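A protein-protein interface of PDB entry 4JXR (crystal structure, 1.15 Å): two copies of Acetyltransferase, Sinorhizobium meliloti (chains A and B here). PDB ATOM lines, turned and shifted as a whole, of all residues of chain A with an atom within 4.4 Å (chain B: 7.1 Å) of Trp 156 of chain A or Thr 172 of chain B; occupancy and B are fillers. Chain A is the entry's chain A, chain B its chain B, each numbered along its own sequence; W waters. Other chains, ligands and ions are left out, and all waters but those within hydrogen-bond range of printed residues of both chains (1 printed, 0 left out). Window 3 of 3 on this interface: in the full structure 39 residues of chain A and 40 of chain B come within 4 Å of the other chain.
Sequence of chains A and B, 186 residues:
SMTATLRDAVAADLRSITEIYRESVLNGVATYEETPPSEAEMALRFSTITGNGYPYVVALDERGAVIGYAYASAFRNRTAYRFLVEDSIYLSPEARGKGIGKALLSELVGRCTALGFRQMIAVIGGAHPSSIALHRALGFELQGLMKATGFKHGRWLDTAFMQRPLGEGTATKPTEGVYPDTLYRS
O of Thr 172 of chain B sits at hydrogen-bond distance from NE1 of Trp 156 of chain A. O of Ala 80 of chain B sits at hydrogen-bond distance from N of Phe 151 of chain A, 2.8 Å away.
The backbone carbonyl oxygen of Leu 157 of chain A lies close to the backbone NH of Ala 148 of chain A. O of Phe 83 of chain B lies within hydrogen-bond range of N of Arg 118 of chain B (2.8 Å). NH1 of Arg 118 of chain B is in hydrogen-bond range of O of Gly 169 of chain B. The side-chain carboxylate of Asp 158 of chain A sits at hydrogen-bond distance from the backbone NH of Ala 148 of chain A. The side-chain carboxylate of Glu 168 of chain B is in hydrogen-bond range of the side-chain hydroxyl of Thr 172 of chain B (2.6 Å). NH1 of Arg 118 of chain B is in hydrogen-bond range of O of Thr 172 of chain B (2.9 Å).
Among the printed residues, merely in contact across the chains: Gly 150 of chain A with Ala 80 of chain B, Ala 148 of chain A with Gln 119 of chain B, Trp 156 of chain A with Thr 170 of chain B, Ala 148 of chain A with Thr 170 of chain B, Trp 156 of chain A with Pro 174 of chain B, Phe 151 of chain A with Pro 174 of chain B, Trp 156 of chain A with Arg 118 of chain B, Trp 156 of chain A with Gly 169 of chain B, Phe 151 of chain A with Phe 83 of chain B, Trp 156 of chain A with Phe 83 of chain B and Phe 151 of chain A with Lys 173 of chain B.
Trp 156 of chain A touches just these residues of chain B: Phe 83 (3.9 Å), Arg 118 (3.8 Å), Gly 169 (3.8 Å), Thr 170 (3.4 Å), Thr 172 (3.0 Å) and Pro 174 (3.6 Å). Thr 172 of chain B touches just one residue of chain A: Trp 156 (3.0 Å). Printed residues of chain A within 4 Å of Phe 83 of chain B: Phe 151 and Trp 156. Of the printed residues of chain B, Ala 148 of chain A touches Gln 119 and Thr 170. Of the printed residues of chain B, Gly 150 of chain A touches Ala 80. The nearest printed residue of chain A that does not touch Thr 172 of chain B is Phe 151 of chain A (6.0 Å). The nearest printed residue of chain B that does not touch Phe 151 of chain A is Thr 172 of chain B (6.0 Å).
Of the 7 printed residues of chain A, 4 touch a printed residue of chain B. Printed residues of chain A that touch a printed residue of chain B: Ala 148, Gly 150, Phe 151 and Trp 156. Of the 15 printed residues of chain B, 9 touch a printed residue of chain A. Hydrophobic or aromatic side chains of chain B within 4 Å of the printed part of chain A: Ala 80, Phe 83 and Pro 174. Along chain B the printed residues that touch a printed residue of chain A span positions 80 to 174.
No position is printed for both chains. Of the 13 pairs that touch across the chains among the printed residues, none has its exchanged pair printed and touching as well.
Water W1 lies within hydrogen-bond range of the side-chain amide nitrogen of Gln 119 of chain B, the backbone carbonyl oxygen of Ala 148 of chain A and the backbone carbonyl oxygen of Gly 169 of chain B.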
ATOM      1  N   ALA A 148       7.737   9.623  11.781  1.00  0.00           N
ATOM      2  CA  ALA A 148       7.674  11.099  11.795  1.00  0.00           C
ATOM      3  C   ALA A 148       8.959  11.711  11.240  1.00  0.00           C
ATOM      4  O   ALA A 148       9.454  12.713  11.757  1.00  0.00           O
ATOM      5  CB  ALA A 148       7.356  11.619  13.186  1.00  0.00           C
ATOM      6  N   GLY A 150       9.302  12.405   7.820  1.00  0.00           N
ATOM      7  CA  GLY A 150       8.962  13.359   6.791  1.00  0.00           C
ATOM      8  C   GLY A 150       7.894  14.346   7.280  1.00  0.00           C
ATOM      9  O   GLY A 150       7.124  14.042   8.180  1.00  0.00           O
ATOM     10  N   PHE A 151       7.845  15.507   6.649  1.00  0.00           N
ATOM     11  CA  PHE A 151       6.795  16.498   6.903  1.00  0.00           C
ATOM     12  C   PHE A 151       6.392  17.051   5.561  1.00  0.00           C
ATOM     13  O   PHE A 151       7.206  17.673   4.907  1.00  0.00           O
ATOM     14  CB  PHE A 151       7.279  17.594   7.857  1.00  0.00           C
ATOM     15  CG  PHE A 151       6.142  18.461   8.315  1.00  0.00           C
ATOM     16  CD1 PHE A 151       5.277  18.012   9.299  1.00  0.00           C
ATOM     17  CD2 PHE A 151       5.891  19.685   7.703  1.00  0.00           C
ATOM     18  CE1 PHE A 151       4.220  18.793   9.710  1.00  0.00           C
ATOM     19  CE2 PHE A 151       4.834  20.476   8.142  1.00  0.00           C
ATOM     20  CZ  PHE A 151       3.987  20.024   9.120  1.00  0.00           C
ATOM     21  N   ARG A 155       1.591  17.377   7.432  1.00  0.00           N
ATOM     22  CA  ARG A 155       1.504  16.164   8.241  1.00  0.00           C
ATOM     23  C   ARG A 155       2.890  15.557   8.475  1.00  0.00           C
ATOM     24  O   ARG A 155       3.722  15.511   7.558  1.00  0.00           O
ATOM     25  CB  ARG A 155       0.660  15.099   7.495  1.00  0.00           C
ATOM     26  CG  ARG A 155      -0.748  15.553   7.122  1.00  0.00           C
ATOM     27  CD  ARG A 155      -1.655  14.403   6.678  1.00  0.00           C
ATOM     28  NE  ARG A 155      -0.957  13.237   6.147  1.00  0.00           N
ATOM     29  CZ  ARG A 155      -0.685  13.046   4.860  1.00  0.00           C
ATOM     30  NH1 ARG A 155      -0.052  11.941   4.469  1.00  0.00           N
ATOM     31  NH2 ARG A 155      -1.041  13.957   3.962  1.00  0.00           N
ATOM     32  N   TRP A 156       3.083  15.006   9.653  1.00  0.00           N
ATOM     33  CA  TRP A 156       4.226  14.121   9.913  1.00  0.00           C
ATOM     34  C   TRP A 156       4.004  12.798   9.209  1.00  0.00           C
ATOM     35  O   TRP A 156       2.926  12.208   9.290  1.00  0.00           O
ATOM     36  CB  TRP A 156       4.436  13.903  11.418  1.00  0.00           C
ATOM     37  CG  TRP A 156       4.943  15.093  12.148  1.00  0.00           C
ATOM     38  CD1 TRP A 156       4.254  15.873  13.077  1.00  0.00           C
ATOM     39  CD2 TRP A 156       6.224  15.692  12.010  1.00  0.00           C
ATOM     40  NE1 TRP A 156       5.048  16.883  13.522  1.00  0.00           N
ATOM     41  CE2 TRP A 156       6.266  16.803  12.878  1.00  0.00           C
ATOM     42  CE3 TRP A 156       7.348  15.420  11.189  1.00  0.00           C
ATOM     43  CZ2 TRP A 156       7.359  17.618  12.986  1.00  0.00           C
ATOM     44  CZ3 TRP A 156       8.432  16.231  11.284  1.00  0.00           C
ATOM     45  CH2 TRP A 156       8.437  17.328  12.188  1.00  0.00           C
ATOM     46  N   LEU A 157       5.037  12.292   8.554  1.00  0.00           N
ATOM     47  CA  LEU A 157       5.019  11.091   7.773  1.00  0.00           C
ATOM     48  C   LEU A 157       6.014  10.101   8.299  1.00  0.00           C
ATOM     49  O   LEU A 157       7.142  10.450   8.634  1.00  0.00           O
ATOM     50  CB  LEU A 157       5.428  11.419   6.330  1.00  0.00           C
ATOM     51  CG  LEU A 157       4.576  12.441   5.580  1.00  0.00           C
ATOM     52  CD1 LEU A 157       5.142  12.636   4.189  1.00  0.00           C
ATOM     53  CD2 LEU A 157       3.154  12.026   5.466  1.00  0.00           C
ATOM     54  N   ASP A 158       5.611   8.846   8.335  1.00  0.00           N
ATOM     55  CA  ASP A 158       6.512   7.726   8.605  1.00  0.00           C
ATOM     56  C   ASP A 158       7.173   7.288   7.297  1.00  0.00           C
ATOM     57  O   ASP A 158       6.589   7.439   6.217  1.00  0.00           O
ATOM     58  CB  ASP A 158       5.754   6.580   9.227  1.00  0.00           C
ATOM     59  CG  ASP A 158       5.074   6.921  10.546  1.00  0.00           C
ATOM     60  OD1 ASP A 158       5.459   7.866  11.230  1.00  0.00           O
ATOM     61  OD2 ASP A 158       4.133   6.149  10.889  1.00  0.00           O
ATOM     62  N   ALA B  80      11.025  17.177   2.420  1.00  0.00           N
ATOM     63  CA  ALA B  80      10.211  16.664   3.502  1.00  0.00           C
ATOM     64  C   ALA B  80      11.039  16.092   4.647  1.00  0.00           C
ATOM     65  O   ALA B  80      10.494  15.927   5.738  1.00  0.00           O
ATOM     66  CB  ALA B  80       9.189  15.671   3.046  1.00  0.00           C
ATOM     67  N   PHE B  83      13.377  18.227   8.857  1.00  0.00           N
ATOM     68  CA  PHE B  83      13.386  18.183  10.310  1.00  0.00           C
ATOM     69  C   PHE B  83      14.109  16.976  10.859  1.00  0.00           C
ATOM     70  O   PHE B  83      14.194  16.817  12.102  1.00  0.00           O
ATOM     71  CB  PHE B  83      11.965  18.273  10.889  1.00  0.00           C
ATOM     72  CG  PHE B  83      11.238  19.493  10.394  1.00  0.00           C
ATOM     73  CD1 PHE B  83      11.531  20.711  10.933  1.00  0.00           C
ATOM     74  CD2 PHE B  83      10.342  19.408   9.377  1.00  0.00           C
ATOM     75  CE1 PHE B  83      10.933  21.877  10.437  1.00  0.00           C
ATOM     76  CE2 PHE B  83       9.728  20.552   8.861  1.00  0.00           C
ATOM     77  CZ  PHE B  83      10.024  21.762   9.429  1.00  0.00           C
ATOM     78  N   LEU B  84      14.673  16.149   9.985  1.00  0.00           N
ATOM     79  CA  LEU B  84      15.440  14.956  10.356  1.00  0.00           C
ATOM     80  C   LEU B  84      16.935  15.232  10.138  1.00  0.00           C
ATOM     81  O   LEU B  84      17.315  15.719   9.048  1.00  0.00           O
ATOM     82  CB  LEU B  84      15.005  13.800   9.458  1.00  0.00           C
ATOM     83  CG  LEU B  84      15.829  12.530   9.522  1.00  0.00           C
ATOM     84  CD1 LEU B  84      15.797  11.881  10.913  1.00  0.00           C
ATOM     85  CD2 LEU B  84      15.379  11.560   8.448  1.00  0.00           C
ATOM     86  N   GLY B 116      15.994  23.224  16.469  1.00  0.00           N
ATOM     87  CA  GLY B 116      14.647  22.999  16.032  1.00  0.00           C
ATOM     88  C   GLY B 116      14.392  21.775  15.216  1.00  0.00           C
ATOM     89  O   GLY B 116      13.299  21.572  14.684  1.00  0.00           O
ATOM     90  N   PHE B 117      15.388  20.895  15.051  1.00  0.00           N
ATOM     91  CA  PHE B 117      15.128  19.603  14.427  1.00  0.00           C
ATOM     92  C   PHE B 117      14.267  18.734  15.342  1.00  0.00           C
ATOM     93  O   PHE B 117      14.197  18.982  16.547  1.00  0.00           O
ATOM     94  CB  PHE B 117      16.477  18.894  14.094  1.00  0.00           C
ATOM     95  CG  PHE B 117      17.318  19.718  13.119  1.00  0.00           C
ATOM     96  CD1 PHE B 117      16.996  19.721  11.777  1.00  0.00           C
ATOM     97  CD2 PHE B 117      18.363  20.468  13.546  1.00  0.00           C
ATOM     98  CE1 PHE B 117      17.732  20.471  10.880  1.00  0.00           C
ATOM     99  CE2 PHE B 117      19.121  21.223  12.651  1.00  0.00           C
ATOM    100  CZ  PHE B 117      18.762  21.226  11.335  1.00  0.00           C
ATOM    101  N   ARG B 118      13.639  17.714  14.741  1.00  0.00           N
ATOM    102  CA  ARG B 118      12.650  16.919  15.454  1.00  0.00           C
ATOM    103  C   ARG B 118      12.950  15.439  15.559  1.00  0.00           C
ATOM    104  O   ARG B 118      12.334  14.757  16.373  1.00  0.00           O
ATOM    105  CB  ARG B 118      11.246  17.136  14.860  1.00  0.00           C
ATOM    106  CG  ARG B 118      10.736  18.560  14.971  1.00  0.00           C
ATOM    107  CD  ARG B 118      10.586  19.027  16.411  1.00  0.00           C
ATOM    108  NE  ARG B 118       9.846  20.280  16.499  1.00  0.00           N
ATOM    109  CZ  ARG B 118       8.529  20.362  16.450  1.00  0.00           C
ATOM    110  NH1 ARG B 118       7.777  19.308  16.340  1.00  0.00           N
ATOM    111  NH2 ARG B 118       7.961  21.568  16.487  1.00  0.00           N
ATOM    112  N   GLN B 119      13.860  14.896  14.730  1.00  0.00           N
ATOM    113  CA  GLN B 119      14.253  13.500  14.803  1.00  0.00           C
ATOM    114  C   GLN B 119      15.718  13.401  14.441  1.00  0.00           C
ATOM    115  O   GLN B 119      16.183  14.164  13.568  1.00  0.00           O
ATOM    116  CB  GLN B 119      13.418  12.613  13.840  1.00  0.00           C
ATOM    117  CG  GLN B 119      11.899  12.685  14.042  1.00  0.00           C
ATOM    118  CD  GLN B 119      11.403  12.013  15.279  1.00  0.00           C
ATOM    119  OE1 GLN B 119      12.015  11.065  15.798  1.00  0.00           O
ATOM    120  NE2 GLN B 119      10.238  12.453  15.738  1.00  0.00           N
ATOM    121  N   GLU B 168      10.274  18.540  20.792  1.00  0.00           N
ATOM    122  CA  GLU B 168       8.853  18.162  20.728  1.00  0.00           C
ATOM    123  C   GLU B 168       8.570  16.962  19.829  1.00  0.00           C
ATOM    124  O   GLU B 168       7.470  16.401  19.886  1.00  0.00           O
ATOM    125  CB  GLU B 168       8.042  19.372  20.321  1.00  0.00           C
ATOM    126  CG  GLU B 168       8.026  20.368  21.461  1.00  0.00           C
ATOM    127  CD  GLU B 168       7.271  21.629  21.211  1.00  0.00           C
ATOM    128  OE1 GLU B 168       6.829  21.925  20.102  1.00  0.00           O
ATOM    129  OE2 GLU B 168       7.145  22.382  22.195  1.00  0.00           O
ATOM    130  N   GLY B 169       9.534  16.521  19.013  1.00  0.00           N
ATOM    131  CA  GLY B 169       9.327  15.354  18.188  1.00  0.00           C
ATOM    132  C   GLY B 169       8.156  15.527  17.278  1.00  0.00           C
ATOM    133  O   GLY B 169       8.018  16.495  16.567  1.00  0.00           O
ATOM    134  N   THR B 170       7.261  14.529  17.267  1.00  0.00           N
ATOM    135  CA  THR B 170       6.096  14.543  16.431  1.00  0.00           C
ATOM    136  C   THR B 170       4.917  15.260  17.091  1.00  0.00           C
ATOM    137  O   THR B 170       3.841  15.318  16.471  1.00  0.00           O
ATOM    138  CB  THR B 170       5.648  13.113  16.086  1.00  0.00           C
ATOM    139  OG1 THR B 170       4.724  13.108  14.999  1.00  0.00           O
ATOM    140  CG2 THR B 170       5.056  12.410  17.335  1.00  0.00           C
ATOM    141  N   ALA B 171       5.052  15.740  18.330  1.00  0.00           N
ATOM    142  CA  ALA B 171       3.883  16.180  19.111  1.00  0.00           C
ATOM    143  C   ALA B 171       3.291  17.500  18.658  1.00  0.00           C
ATOM    144  O   ALA B 171       2.135  17.813  19.019  1.00  0.00           O
ATOM    145  CB  ALA B 171       4.240  16.242  20.561  1.00  0.00           C
ATOM    146  N   THR B 172       4.062  18.333  17.997  1.00  0.00           N
ATOM    147  CA  THR B 172       3.610  19.617  17.508  1.00  0.00           C
ATOM    148  C   THR B 172       4.026  19.749  16.077  1.00  0.00           C
ATOM    149  O   THR B 172       4.985  19.067  15.613  1.00  0.00           O
ATOM    150  CB  THR B 172       4.173  20.806  18.300  1.00  0.00           C
ATOM    151  OG1 THR B 172       5.598  20.785  18.128  1.00  0.00           O
ATOM    152  CG2 THR B 172       3.775  20.741  19.755  1.00  0.00           C
ATOM    153  N   LYS B 173       3.421  20.656  15.359  1.00  0.00           N
ATOM    154  CA  LYS B 173       3.807  20.995  14.026  1.00  0.00           C
ATOM    155  C   LYS B 173       5.029  21.900  14.099  1.00  0.00           C
ATOM    156  O   LYS B 173       5.179  22.670  15.062  1.00  0.00           O
ATOM    157  CB  LYS B 173       2.693  21.710  13.277  1.00  0.00           C
ATOM    158  CG  LYS B 173       1.407  20.894  13.203  1.00  0.00           C
ATOM    159  CD  LYS B 173       1.619  19.536  12.559  1.00  0.00           C
ATOM    160  CE  LYS B 173       0.353  18.694  12.481  1.00  0.00           C
ATOM    161  NZ  LYS B 173      -0.613  19.301  11.534  1.00  0.00           N
ATOM    162  N   PRO B 174       5.937  21.876  13.098  1.00  0.00           N
ATOM    163  CA  PRO B 174       7.075  22.805  13.201  1.00  0.00           C
ATOM    164  C   PRO B 174       6.649  24.275  13.039  1.00  0.00           C
ATOM    165  O   PRO B 174       5.666  24.550  12.389  1.00  0.00           O
ATOM    166  CB  PRO B 174       7.989  22.388  12.058  1.00  0.00           C
ATOM    167  CG  PRO B 174       7.599  21.003  11.788  1.00  0.00           C
ATOM    168  CD  PRO B 174       6.132  20.870  12.037  1.00  0.00           C
ATOM    169  N   THR B 175       7.492  25.193  13.525  1.00  0.00           N
ATOM    170  CA  THR B 175       7.301  26.633  13.339  1.00  0.00           C
ATOM    171  C   THR B 175       7.664  26.992  11.935  1.00  0.00           C
ATOM    172  O   THR B 175       8.819  26.823  11.518  1.00  0.00           O
ATOM    173  CB  THR B 175       8.148  27.443  14.329  1.00  0.00           C
ATOM    174  OG1 THR B 175       7.846  27.008  15.670  1.00  0.00           O
ATOM    175  CG2 THR B 175       7.842  28.916  14.162  1.00  0.00           C
HETATM  176  O   HOH W   1       8.973  14.479  14.115  1.00  0.00           O
